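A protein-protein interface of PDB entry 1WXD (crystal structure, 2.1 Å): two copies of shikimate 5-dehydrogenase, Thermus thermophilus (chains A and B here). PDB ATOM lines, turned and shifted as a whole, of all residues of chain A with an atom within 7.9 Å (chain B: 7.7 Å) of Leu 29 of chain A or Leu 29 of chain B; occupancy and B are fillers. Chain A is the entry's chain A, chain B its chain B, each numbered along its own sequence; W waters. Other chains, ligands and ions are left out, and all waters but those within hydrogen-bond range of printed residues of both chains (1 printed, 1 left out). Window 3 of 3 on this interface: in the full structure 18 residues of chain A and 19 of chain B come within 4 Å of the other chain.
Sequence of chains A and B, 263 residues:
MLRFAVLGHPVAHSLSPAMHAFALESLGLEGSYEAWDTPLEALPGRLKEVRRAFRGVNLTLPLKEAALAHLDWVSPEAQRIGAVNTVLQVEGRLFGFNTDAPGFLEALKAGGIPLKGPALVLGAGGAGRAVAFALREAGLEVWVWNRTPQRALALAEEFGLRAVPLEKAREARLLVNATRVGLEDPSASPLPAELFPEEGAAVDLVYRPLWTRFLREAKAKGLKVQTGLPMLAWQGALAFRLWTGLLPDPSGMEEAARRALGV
O of Leu 24 of chain A lies within hydrogen-bond range of N of Leu 29 of chain A, at 2.8 Å. The backbone NH of Ser 32 of chain B lies within hydrogen-bond range of the backbone carbonyl oxygen of Leu 2 of chain B. The side-chain hydroxyl (OG1) of Thr 244 of chain B lies close to the backbone NH (N) of Leu 246 of chain B (3.3 Å). The backbone carbonyl oxygen of Glu 30 of chain B lies within hydrogen-bond range of the backbone NH of Leu 2 of chain B (3.1 Å). The backbone NH (N) of Leu 246 of chain A sits at hydrogen-bond distance from the side-chain hydroxyl (OG1) of Thr 244 of chain A (3.1 Å). N of Ser 32 of chain A lies within hydrogen-bond range of O of Leu 2 of chain A (3.2 Å).
Among the printed residues, pairs that only touch across the chains: Met 1 of chain A with Leu 246 of chain B (3.8 Å), Leu 2 of chain A with Thr 244 of chain B (3.7 Å), Leu 2 of chain A with Leu 246 of chain B (3.4 Å), Leu 29 of chain A with Leu 29 of chain B (3.998 Å), Leu 29 of chain A with Leu 246 of chain B (3.9 Å), Thr 244 of chain A with Leu 2 of chain B (3.9 Å), Thr 244 of chain A with Thr 244 of chain B (3.5 Å) and Leu 246 of chain A with Leu 2 of chain B (3.97 Å).
Of the printed residues of chain B, Leu 29 of chain A touches Leu 29 and Leu 246. Printed residues of chain A within 4 Å of Leu 29 of chain B: Leu 29. No residue of chain B comes within 4 Å of Gly 28 of chain A. No residue of chain A comes within 4 Å of Gly 28 of chain B. Printed residues of chain B within 4 Å of Leu 2 of chain A: Thr 244 and Leu 246. Of the printed residues of chain A, Leu 246 of chain B touches Met 1, Leu 2 and Leu 29. Of the printed residues of chain A, Leu 2 of chain B touches Thr 244 (3.9 Å) and Leu 246 (3.97 Å). Of the printed residues of chain B, Thr 244 of chain A touches Leu 2 (3.9 Å) and Thr 244 (3.5 Å). His 20 of chain B touches none of the printed residues of chain A. The nearest printed residue of chain A that does not touch Leu 29 of chain B is Leu 246 of chain A (4.1 Å).
Of the 19 printed residues of chain B, 4 touch a printed residue of chain A. Printed residues of chain B that touch a printed residue of chain A: Leu 2, Leu 29, Thr 244 and Leu 246. Hydrophobic or aromatic side chains of chain B that line the printed part of chain A: Leu 2, Leu 29 and Leu 246. Hydrophobic or aromatic side chains of chain A that line the printed part of chain B: Met 1, Leu 2, Leu 29 and Leu 246. Among the printed residues, no Asp or Glu carboxylate lies within 4 Å of a Lys or Arg side-chain nitrogen of the other chain.
Met 1 of chain A touches Leu 246 of chain B, but with the chains exchanged Leu 246 of chain A does not touch Met 1 of chain B (5.9 Å). Leu 2 of chain A touches Leu 246 of chain B, and with the chains exchanged Leu 246 of chain A touches Leu 2 of chain B. Leu 29 of chain B touches its own counterpart, Leu 29 of chain A. Leu 29 of chain A touches Leu 246 of chain B, but with the chains exchanged Leu 246 of chain A does not touch Leu 29 of chain B (4.1 Å). 19 positions are printed for both chains.
Water W1 bridges the backbone carbonyl oxygen of Leu 27 of chain B and the backbone carbonyl oxygen of Gly 28 of chain A.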
ATOM      1  N   MET A   1      -6.934   6.889  22.034  1.00  0.00           N
ATOM      2  CA  MET A   1      -7.159   5.425  22.173  1.00  0.00           C
ATOM      3  C   MET A   1      -7.985   5.060  23.389  1.00  0.00           C
ATOM      4  O   MET A   1      -7.731   5.521  24.497  1.00  0.00           O
ATOM      5  CB  MET A   1      -5.834   4.682  22.284  1.00  0.00           C
ATOM      6  CG  MET A   1      -4.852   4.935  21.180  1.00  0.00           C
ATOM      7  SD  MET A   1      -3.416   3.907  21.421  1.00  0.00           S
ATOM      8  CE  MET A   1      -2.673   4.678  22.863  1.00  0.00           C
ATOM      9  N   LEU A   2      -8.985   4.224  23.166  1.00  0.00           N
ATOM     10  CA  LEU A   2      -9.838   3.747  24.239  1.00  0.00           C
ATOM     11  C   LEU A   2     -10.557   4.786  25.073  1.00  0.00           C
ATOM     12  O   LEU A   2     -10.183   5.046  26.217  1.00  0.00           O
ATOM     13  CB  LEU A   2      -9.034   2.848  25.169  1.00  0.00           C
ATOM     14  CG  LEU A   2      -8.352   1.677  24.463  1.00  0.00           C
ATOM     15  CD1 LEU A   2      -7.793   0.733  25.509  1.00  0.00           C
ATOM     16  CD2 LEU A   2      -9.348   0.951  23.564  1.00  0.00           C
ATOM     17  N   PHE A   4     -14.366   5.470  26.287  1.00  0.00           N
ATOM     18  CA  PHE A   4     -15.697   4.902  26.308  1.00  0.00           C
ATOM     19  C   PHE A   4     -16.614   5.809  27.110  1.00  0.00           C
ATOM     20  O   PHE A   4     -16.190   6.844  27.624  1.00  0.00           O
ATOM     21  CB  PHE A   4     -15.666   3.510  26.939  1.00  0.00           C
ATOM     22  CG  PHE A   4     -14.592   2.611  26.389  1.00  0.00           C
ATOM     23  CD1 PHE A   4     -13.348   2.538  27.003  1.00  0.00           C
ATOM     24  CD2 PHE A   4     -14.835   1.815  25.275  1.00  0.00           C
ATOM     25  CE1 PHE A   4     -12.362   1.677  26.520  1.00  0.00           C
ATOM     26  CE2 PHE A   4     -13.856   0.955  24.784  1.00  0.00           C
ATOM     27  CZ  PHE A   4     -12.616   0.886  25.410  1.00  0.00           C
ATOM     28  N   HIS A  20     -15.320   0.177  34.764  1.00  0.00           N
ATOM     29  CA  HIS A  20     -14.424   0.254  33.624  1.00  0.00           C
ATOM     30  C   HIS A  20     -13.090   0.920  33.935  1.00  0.00           C
ATOM     31  O   HIS A  20     -12.061   0.564  33.347  1.00  0.00           O
ATOM     32  CB  HIS A  20     -15.147   0.940  32.466  1.00  0.00           C
ATOM     33  CG  HIS A  20     -16.248   0.106  31.882  1.00  0.00           C
ATOM     34  ND1 HIS A  20     -16.017  -0.886  30.954  1.00  0.00           N
ATOM     35  CD2 HIS A  20     -17.576   0.071  32.147  1.00  0.00           C
ATOM     36  CE1 HIS A  20     -17.155  -1.498  30.673  1.00  0.00           C
ATOM     37  NE2 HIS A  20     -18.117  -0.938  31.383  1.00  0.00           N
ATOM     38  N   ALA A  21     -13.091   1.877  34.860  1.00  0.00           N
ATOM     39  CA  ALA A  21     -11.841   2.522  35.246  1.00  0.00           C
ATOM     40  C   ALA A  21     -10.971   1.393  35.779  1.00  0.00           C
ATOM     41  O   ALA A  21      -9.773   1.330  35.506  1.00  0.00           O
ATOM     42  CB  ALA A  21     -12.083   3.558  36.332  1.00  0.00           C
ATOM     43  N   PHE A  22     -11.596   0.487  36.530  1.00  0.00           N
ATOM     44  CA  PHE A  22     -10.891  -0.658  37.091  1.00  0.00           C
ATOM     45  C   PHE A  22     -10.469  -1.653  36.015  1.00  0.00           C
ATOM     46  O   PHE A  22      -9.414  -2.271  36.122  1.00  0.00           O
ATOM     47  CB  PHE A  22     -11.762  -1.380  38.124  1.00  0.00           C
ATOM     48  CG  PHE A  22     -11.310  -2.783  38.408  1.00  0.00           C
ATOM     49  CD1 PHE A  22     -11.810  -3.848  37.667  1.00  0.00           C
ATOM     50  CD2 PHE A  22     -10.332  -3.031  39.364  1.00  0.00           C
ATOM     51  CE1 PHE A  22     -11.339  -5.139  37.868  1.00  0.00           C
ATOM     52  CE2 PHE A  22      -9.853  -4.317  39.575  1.00  0.00           C
ATOM     53  CZ  PHE A  22     -10.357  -5.375  38.825  1.00  0.00           C
ATOM     54  N   ALA A  23     -11.308  -1.820  34.994  1.00  0.00           N
ATOM     55  CA  ALA A  23     -11.012  -2.740  33.901  1.00  0.00           C
ATOM     56  C   ALA A  23      -9.722  -2.309  33.215  1.00  0.00           C
ATOM     57  O   ALA A  23      -8.772  -3.085  33.110  1.00  0.00           O
ATOM     58  CB  ALA A  23     -12.162  -2.750  32.893  1.00  0.00           C
ATOM     59  N   LEU A  24      -9.704  -1.065  32.748  1.00  0.00           N
ATOM     60  CA  LEU A  24      -8.539  -0.501  32.077  1.00  0.00           C
ATOM     61  C   LEU A  24      -7.281  -0.630  32.932  1.00  0.00           C
ATOM     62  O   LEU A  24      -6.255  -1.140  32.476  1.00  0.00           O
ATOM     63  CB  LEU A  24      -8.792   0.977  31.755  1.00  0.00           C
ATOM     64  CG  LEU A  24      -9.839   1.275  30.676  1.00  0.00           C
ATOM     65  CD1 LEU A  24     -10.270   2.732  30.755  1.00  0.00           C
ATOM     66  CD2 LEU A  24      -9.258   0.949  29.299  1.00  0.00           C
ATOM     67  N   GLU A  25      -7.369  -0.176  34.178  1.00  0.00           N
ATOM     68  CA  GLU A  25      -6.237  -0.226  35.094  1.00  0.00           C
ATOM     69  C   GLU A  25      -5.754  -1.652  35.352  1.00  0.00           C
ATOM     70  O   GLU A  25      -4.560  -1.932  35.254  1.00  0.00           O
ATOM     71  CB  GLU A  25      -6.611   0.455  36.419  1.00  0.00           C
ATOM     72  CG  GLU A  25      -5.445   0.674  37.376  1.00  0.00           C
ATOM     73  CD  GLU A  25      -5.056  -0.579  38.143  1.00  0.00           C
ATOM     74  OE1 GLU A  25      -4.029  -0.544  38.855  1.00  0.00           O
ATOM     75  OE2 GLU A  25      -5.777  -1.592  38.047  1.00  0.00           O
ATOM     76  N   SER A  26      -6.679  -2.549  35.681  1.00  0.00           N
ATOM     77  CA  SER A  26      -6.325  -3.938  35.959  1.00  0.00           C
ATOM     78  C   SER A  26      -5.661  -4.598  34.759  1.00  0.00           C
ATOM     79  O   SER A  26      -4.935  -5.576  34.906  1.00  0.00           O
ATOM     80  CB  SER A  26      -7.571  -4.743  36.358  1.00  0.00           C
ATOM     81  OG  SER A  26      -8.460  -4.910  35.266  1.00  0.00           O
ATOM     82  N   LEU A  27      -5.919  -4.058  33.572  1.00  0.00           N
ATOM     83  CA  LEU A  27      -5.354  -4.590  32.336  1.00  0.00           C
ATOM     84  C   LEU A  27      -4.154  -3.769  31.855  1.00  0.00           C
ATOM     85  O   LEU A  27      -3.617  -4.011  30.775  1.00  0.00           O
ATOM     86  CB  LEU A  27      -6.430  -4.615  31.247  1.00  0.00           C
ATOM     87  CG  LEU A  27      -7.603  -5.572  31.471  1.00  0.00           C
ATOM     88  CD1 LEU A  27      -8.659  -5.349  30.408  1.00  0.00           C
ATOM     89  CD2 LEU A  27      -7.104  -7.009  31.439  1.00  0.00           C
ATOM     90  N   GLY A  28      -3.738  -2.797  32.660  1.00  0.00           N
ATOM     91  CA  GLY A  28      -2.605  -1.970  32.287  1.00  0.00           C
ATOM     92  C   GLY A  28      -2.851  -1.233  30.988  1.00  0.00           C
ATOM     93  O   GLY A  28      -1.979  -1.163  30.124  1.00  0.00           O
ATOM     94  N   LEU A  29      -4.052  -0.686  30.848  1.00  0.00           N
ATOM     95  CA  LEU A  29      -4.412   0.053  29.645  1.00  0.00           C
ATOM     96  C   LEU A  29      -4.732   1.500  29.988  1.00  0.00           C
ATOM     97  O   LEU A  29      -5.251   1.790  31.063  1.00  0.00           O
ATOM     98  CB  LEU A  29      -5.635  -0.582  28.980  1.00  0.00           C
ATOM     99  CG  LEU A  29      -5.482  -2.007  28.453  1.00  0.00           C
ATOM    100  CD1 LEU A  29      -6.831  -2.545  27.993  1.00  0.00           C
ATOM    101  CD2 LEU A  29      -4.485  -2.008  27.313  1.00  0.00           C
ATOM    102  N   GLU A  30      -4.413   2.403  29.069  1.00  0.00           N
ATOM    103  CA  GLU A  30      -4.698   3.816  29.260  1.00  0.00           C
ATOM    104  C   GLU A  30      -6.012   4.106  28.565  1.00  0.00           C
ATOM    105  O   GLU A  30      -6.262   3.616  27.464  1.00  0.00           O
ATOM    106  CB  GLU A  30      -3.596   4.688  28.653  1.00  0.00           C
ATOM    107  CG  GLU A  30      -2.296   4.681  29.437  1.00  0.00           C
ATOM    108  CD  GLU A  30      -2.486   5.133  30.875  1.00  0.00           C
ATOM    109  OE1 GLU A  30      -2.995   6.255  31.090  1.00  0.00           O
ATOM    110  OE2 GLU A  30      -2.125   4.363  31.790  1.00  0.00           O
ATOM    111  N   GLY A  31      -6.856   4.898  29.210  1.00  0.00           N
ATOM    112  CA  GLY A  31      -8.135   5.225  28.616  1.00  0.00           C
ATOM    113  C   GLY A  31      -9.081   5.837  29.621  1.00  0.00           C
ATOM    114  O   GLY A  31      -8.695   6.133  30.749  1.00  0.00           O
ATOM    115  N   SER A  32     -10.330   6.020  29.213  1.00  0.00           N
ATOM    116  CA  SER A  32     -11.328   6.612  30.087  1.00  0.00           C
ATOM    117  C   SER A  32     -12.724   6.120  29.745  1.00  0.00           C
ATOM    118  O   SER A  32     -12.974   5.636  28.643  1.00  0.00           O
ATOM    119  CB  SER A  32     -11.284   8.132  29.961  1.00  0.00           C
ATOM    120  OG  SER A  32     -11.572   8.522  28.630  1.00  0.00           O
ATOM    121  N   PHE A 240     -16.550  -4.921  27.470  1.00  0.00           N
ATOM    122  CA  PHE A 240     -15.135  -4.562  27.387  1.00  0.00           C
ATOM    123  C   PHE A 240     -14.390  -5.493  26.432  1.00  0.00           C
ATOM    124  O   PHE A 240     -13.537  -5.048  25.662  1.00  0.00           O
ATOM    125  CB  PHE A 240     -14.470  -4.625  28.766  1.00  0.00           C
ATOM    126  CG  PHE A 240     -13.211  -3.799  28.865  1.00  0.00           C
ATOM    127  CD1 PHE A 240     -13.279  -2.446  29.170  1.00  0.00           C
ATOM    128  CD2 PHE A 240     -11.962  -4.361  28.606  1.00  0.00           C
ATOM    129  CE1 PHE A 240     -12.132  -1.659  29.214  1.00  0.00           C
ATOM    130  CE2 PHE A 240     -10.806  -3.581  28.647  1.00  0.00           C
ATOM    131  CZ  PHE A 240     -10.894  -2.223  28.954  1.00  0.00           C
ATOM    132  N   THR A 244     -12.323  -4.489  23.107  1.00  0.00           N
ATOM    133  CA  THR A 244     -10.885  -4.682  23.006  1.00  0.00           C
ATOM    134  C   THR A 244     -10.380  -6.085  22.729  1.00  0.00           C
ATOM    135  O   THR A 244      -9.280  -6.246  22.197  1.00  0.00           O
ATOM    136  CB  THR A 244     -10.205  -4.213  24.290  1.00  0.00           C
ATOM    137  OG1 THR A 244     -10.545  -5.111  25.356  1.00  0.00           O
ATOM    138  CG2 THR A 244     -10.670  -2.806  24.653  1.00  0.00           C
ATOM    139  N   LEU A 246     -10.237  -8.180  25.258  1.00  0.00           N
ATOM    140  CA  LEU A 246      -9.738  -8.553  26.579  1.00  0.00           C
ATOM    141  C   LEU A 246     -10.896  -8.625  27.562  1.00  0.00           C
ATOM    142  O   LEU A 246     -11.791  -7.780  27.533  1.00  0.00           O
ATOM    143  CB  LEU A 246      -8.729  -7.516  27.073  1.00  0.00           C
ATOM    144  CG  LEU A 246      -7.508  -7.269  26.190  1.00  0.00           C
ATOM    145  CD1 LEU A 246      -6.750  -6.061  26.711  1.00  0.00           C
ATOM    146  CD2 LEU A 246      -6.622  -8.502  26.175  1.00  0.00           C
ATOM    147  N   MET B   1      -5.440 -14.480  25.972  1.00  0.00           N
ATOM    148  CA  MET B   1      -4.440 -13.908  25.029  1.00  0.00           C
ATOM    149  C   MET B   1      -5.045 -13.565  23.677  1.00  0.00           C
ATOM    150  O   MET B   1      -5.819 -14.345  23.116  1.00  0.00           O
ATOM    151  CB  MET B   1      -3.289 -14.893  24.824  1.00  0.00           C
ATOM    152  CG  MET B   1      -2.300 -14.932  25.969  1.00  0.00           C
ATOM    153  SD  MET B   1      -1.001 -16.132  25.679  1.00  0.00           S
ATOM    154  CE  MET B   1      -0.424 -15.614  24.069  1.00  0.00           C
ATOM    155  N   LEU B   2      -4.693 -12.390  23.163  1.00  0.00           N
ATOM    156  CA  LEU B   2      -5.180 -11.955  21.862  1.00  0.00           C
ATOM    157  C   LEU B   2      -4.561 -12.894  20.832  1.00  0.00           C
ATOM    158  O   LEU B   2      -3.348 -13.117  20.847  1.00  0.00           O
ATOM    159  CB  LEU B   2      -4.744 -10.511  21.589  1.00  0.00           C
ATOM    160  CG  LEU B   2      -5.309  -9.466  22.560  1.00  0.00           C
ATOM    161  CD1 LEU B   2      -4.573  -8.140  22.419  1.00  0.00           C
ATOM    162  CD2 LEU B   2      -6.795  -9.292  22.292  1.00  0.00           C
ATOM    163  N   PHE B   4      -4.032 -13.542  16.823  1.00  0.00           N
ATOM    164  CA  PHE B   4      -4.107 -13.013  15.469  1.00  0.00           C
ATOM    165  C   PHE B   4      -3.322 -13.890  14.495  1.00  0.00           C
ATOM    166  O   PHE B   4      -2.546 -14.760  14.900  1.00  0.00           O
ATOM    167  CB  PHE B   4      -3.526 -11.595  15.408  1.00  0.00           C
ATOM    168  CG  PHE B   4      -4.158 -10.628  16.363  1.00  0.00           C
ATOM    169  CD1 PHE B   4      -3.453 -10.171  17.473  1.00  0.00           C
ATOM    170  CD2 PHE B   4      -5.444 -10.152  16.143  1.00  0.00           C
ATOM    171  CE1 PHE B   4      -4.021  -9.246  18.349  1.00  0.00           C
ATOM    172  CE2 PHE B   4      -6.023  -9.229  17.010  1.00  0.00           C
ATOM    173  CZ  PHE B   4      -5.311  -8.774  18.116  1.00  0.00           C
ATOM    174  N   HIS B  20       3.307  -6.943  13.924  1.00  0.00           N
ATOM    175  CA  HIS B  20       2.347  -7.138  14.992  1.00  0.00           C
ATOM    176  C   HIS B  20       2.989  -7.654  16.278  1.00  0.00           C
ATOM    177  O   HIS B  20       2.494  -7.391  17.373  1.00  0.00           O
ATOM    178  CB  HIS B  20       1.228  -8.034  14.483  1.00  0.00           C
ATOM    179  CG  HIS B  20       0.415  -7.385  13.409  1.00  0.00           C
ATOM    180  ND1 HIS B  20      -0.557  -6.446  13.681  1.00  0.00           N
ATOM    181  CD2 HIS B  20       0.488  -7.467  12.060  1.00  0.00           C
ATOM    182  CE1 HIS B  20      -1.046  -5.978  12.547  1.00  0.00           C
ATOM    183  NE2 HIS B  20      -0.428  -6.581  11.549  1.00  0.00           N
ATOM    184  N   ALA B  21       4.101  -8.369  16.148  1.00  0.00           N
ATOM    185  CA  ALA B  21       4.820  -8.844  17.322  1.00  0.00           C
ATOM    186  C   ALA B  21       5.268  -7.578  18.053  1.00  0.00           C
ATOM    187  O   ALA B  21       5.122  -7.464  19.269  1.00  0.00           O
ATOM    188  CB  ALA B  21       6.025  -9.666  16.905  1.00  0.00           C
ATOM    189  N   PHE B  22       5.815  -6.623  17.303  1.00  0.00           N
ATOM    190  CA  PHE B  22       6.247  -5.362  17.897  1.00  0.00           C
ATOM    191  C   PHE B  22       5.043  -4.612  18.471  1.00  0.00           C
ATOM    192  O   PHE B  22       5.141  -3.982  19.522  1.00  0.00           O
ATOM    193  CB  PHE B  22       6.949  -4.480  16.858  1.00  0.00           C
ATOM    194  CG  PHE B  22       6.900  -3.014  17.180  1.00  0.00           C
ATOM    195  CD1 PHE B  22       5.864  -2.220  16.698  1.00  0.00           C
ATOM    196  CD2 PHE B  22       7.856  -2.437  18.008  1.00  0.00           C
ATOM    197  CE1 PHE B  22       5.778  -0.871  17.038  1.00  0.00           C
ATOM    198  CE2 PHE B  22       7.780  -1.088  18.357  1.00  0.00           C
ATOM    199  CZ  PHE B  22       6.735  -0.303  17.869  1.00  0.00           C
ATOM    200  N   ALA B  23       3.914  -4.663  17.771  1.00  0.00           N
ATOM    201  CA  ALA B  23       2.717  -3.986  18.257  1.00  0.00           C
ATOM    202  C   ALA B  23       2.346  -4.563  19.620  1.00  0.00           C
ATOM    203  O   ALA B  23       2.146  -3.827  20.585  1.00  0.00           O
ATOM    204  CB  ALA B  23       1.567  -4.181  17.282  1.00  0.00           C
ATOM    205  N   LEU B  24       2.267  -5.888  19.697  1.00  0.00           N
ATOM    206  CA  LEU B  24       1.909  -6.536  20.949  1.00  0.00           C
ATOM    207  C   LEU B  24       2.838  -6.137  22.094  1.00  0.00           C
ATOM    208  O   LEU B  24       2.380  -5.644  23.129  1.00  0.00           O
ATOM    209  CB  LEU B  24       1.903  -8.058  20.775  1.00  0.00           C
ATOM    210  CG  LEU B  24       0.691  -8.584  19.996  1.00  0.00           C
ATOM    211  CD1 LEU B  24       0.907 -10.020  19.564  1.00  0.00           C
ATOM    212  CD2 LEU B  24      -0.552  -8.471  20.872  1.00  0.00           C
ATOM    213  N   GLU B  25       4.141  -6.319  21.894  1.00  0.00           N
ATOM    214  CA  GLU B  25       5.087  -5.985  22.944  1.00  0.00           C
ATOM    215  C   GLU B  25       5.130  -4.507  23.282  1.00  0.00           C
ATOM    216  O   GLU B  25       5.134  -4.145  24.460  1.00  0.00           O
ATOM    217  CB  GLU B  25       6.499  -6.471  22.615  1.00  0.00           C
ATOM    218  CG  GLU B  25       7.484  -6.162  23.726  1.00  0.00           C
ATOM    219  CD  GLU B  25       8.600  -7.179  23.809  1.00  0.00           C
ATOM    220  OE1 GLU B  25       9.526  -7.092  22.976  1.00  0.00           O
ATOM    221  OE2 GLU B  25       8.558  -8.055  24.707  1.00  0.00           O
ATOM    222  N   SER B  26       5.154  -3.653  22.264  1.00  0.00           N
ATOM    223  CA  SER B  26       5.193  -2.212  22.483  1.00  0.00           C
ATOM    224  C   SER B  26       3.983  -1.749  23.297  1.00  0.00           C
ATOM    225  O   SER B  26       4.101  -0.891  24.168  1.00  0.00           O
ATOM    226  CB  SER B  26       5.220  -1.462  21.143  1.00  0.00           C
ATOM    227  OG  SER B  26       3.976  -1.552  20.474  1.00  0.00           O
ATOM    228  N   LEU B  27       2.819  -2.324  23.020  1.00  0.00           N
ATOM    229  CA  LEU B  27       1.604  -1.939  23.732  1.00  0.00           C
ATOM    230  C   LEU B  27       1.397  -2.717  25.032  1.00  0.00           C
ATOM    231  O   LEU B  27       0.367  -2.573  25.693  1.00  0.00           O
ATOM    232  CB  LEU B  27       0.391  -2.108  22.813  1.00  0.00           C
ATOM    233  CG  LEU B  27       0.476  -1.241  21.551  1.00  0.00           C
ATOM    234  CD1 LEU B  27      -0.598  -1.643  20.558  1.00  0.00           C
ATOM    235  CD2 LEU B  27       0.348   0.227  21.930  1.00  0.00           C
ATOM    236  N   GLY B  28       2.381  -3.532  25.396  1.00  0.00           N
ATOM    237  CA  GLY B  28       2.289  -4.303  26.623  1.00  0.00           C
ATOM    238  C   GLY B  28       1.117  -5.268  26.680  1.00  0.00           C
ATOM    239  O   GLY B  28       0.524  -5.475  27.736  1.00  0.00           O
ATOM    240  N   LEU B  29       0.791  -5.877  25.547  1.00  0.00           N
ATOM    241  CA  LEU B  29      -0.317  -6.827  25.468  1.00  0.00           C
ATOM    242  C   LEU B  29       0.206  -8.243  25.307  1.00  0.00           C
ATOM    243  O   LEU B  29       1.259  -8.459  24.704  1.00  0.00           O
ATOM    244  CB  LEU B  29      -1.211  -6.504  24.266  1.00  0.00           C
ATOM    245  CG  LEU B  29      -1.892  -5.136  24.189  1.00  0.00           C
ATOM    246  CD1 LEU B  29      -2.360  -4.906  22.762  1.00  0.00           C
ATOM    247  CD2 LEU B  29      -3.059  -5.058  25.157  1.00  0.00           C
ATOM    248  N   GLU B  30      -0.526  -9.206  25.853  1.00  0.00           N
ATOM    249  CA  GLU B  30      -0.141 -10.607  25.738  1.00  0.00           C
ATOM    250  C   GLU B  30      -0.934 -11.264  24.616  1.00  0.00           C
ATOM    251  O   GLU B  30      -2.165 -11.235  24.612  1.00  0.00           O
ATOM    252  CB  GLU B  30      -0.390 -11.342  27.057  1.00  0.00           C
ATOM    253  CG  GLU B  30       0.711 -11.136  28.081  1.00  0.00           C
ATOM    254  CD  GLU B  30       2.053 -11.662  27.597  1.00  0.00           C
ATOM    255  OE1 GLU B  30       2.160 -12.883  27.351  1.00  0.00           O
ATOM    256  OE2 GLU B  30       2.999 -10.857  27.454  1.00  0.00           O
ATOM    257  N   GLY B  31      -0.219 -11.843  23.659  1.00  0.00           N
ATOM    258  CA  GLY B  31      -0.875 -12.496  22.543  1.00  0.00           C
ATOM    259  C   GLY B  31       0.122 -12.853  21.464  1.00  0.00           C
ATOM    260  O   GLY B  31       1.324 -12.686  21.649  1.00  0.00           O
ATOM    261  N   SER B  32      -0.376 -13.341  20.332  1.00  0.00           N
ATOM    262  CA  SER B  32       0.490 -13.721  19.228  1.00  0.00           C
ATOM    263  C   SER B  32      -0.150 -13.453  17.870  1.00  0.00           C
ATOM    264  O   SER B  32      -1.369 -13.362  17.751  1.00  0.00           O
ATOM    265  CB  SER B  32       0.833 -15.205  19.327  1.00  0.00           C
ATOM    266  OG  SER B  32      -0.336 -15.988  19.168  1.00  0.00           O
ATOM    267  N   PHE B 240      -4.535  -3.366  13.605  1.00  0.00           N
ATOM    268  CA  PHE B 240      -4.408  -3.628  15.032  1.00  0.00           C
ATOM    269  C   PHE B 240      -5.411  -2.778  15.812  1.00  0.00           C
ATOM    270  O   PHE B 240      -6.060  -3.263  16.744  1.00  0.00           O
ATOM    271  CB  PHE B 240      -2.993  -3.318  15.522  1.00  0.00           C
ATOM    272  CG  PHE B 240      -2.672  -3.949  16.843  1.00  0.00           C
ATOM    273  CD1 PHE B 240      -2.159  -5.240  16.902  1.00  0.00           C
ATOM    274  CD2 PHE B 240      -2.938  -3.280  18.032  1.00  0.00           C
ATOM    275  CE1 PHE B 240      -1.918  -5.858  18.133  1.00  0.00           C
ATOM    276  CE2 PHE B 240      -2.702  -3.885  19.262  1.00  0.00           C
ATOM    277  CZ  PHE B 240      -2.191  -5.176  19.313  1.00  0.00           C
ATOM    278  N   THR B 244      -8.172  -4.094  18.517  1.00  0.00           N
ATOM    279  CA  THR B 244      -8.144  -3.787  19.946  1.00  0.00           C
ATOM    280  C   THR B 244      -8.465  -2.348  20.343  1.00  0.00           C
ATOM    281  O   THR B 244      -8.701  -2.068  21.517  1.00  0.00           O
ATOM    282  CB  THR B 244      -6.761  -4.120  20.549  1.00  0.00           C
ATOM    283  OG1 THR B 244      -5.789  -3.188  20.057  1.00  0.00           O
ATOM    284  CG2 THR B 244      -6.334  -5.532  20.167  1.00  0.00           C
ATOM    285  N   LEU B 246      -6.333   0.047  19.999  1.00  0.00           N
ATOM    286  CA  LEU B 246      -5.052   0.684  20.295  1.00  0.00           C
ATOM    287  C   LEU B 246      -4.230   0.735  19.005  1.00  0.00           C
ATOM    288  O   LEU B 246      -4.182  -0.241  18.256  1.00  0.00           O
ATOM    289  CB  LEU B 246      -4.280  -0.117  21.352  1.00  0.00           C
ATOM    290  CG  LEU B 246      -4.913  -0.366  22.722  1.00  0.00           C
ATOM    291  CD1 LEU B 246      -4.028  -1.306  23.520  1.00  0.00           C
ATOM    292  CD2 LEU B 246      -5.089   0.945  23.458  1.00  0.00           C
HETATM  293  O   HOH W   1      -1.245  -0.981  27.120  1.00  0.00           O
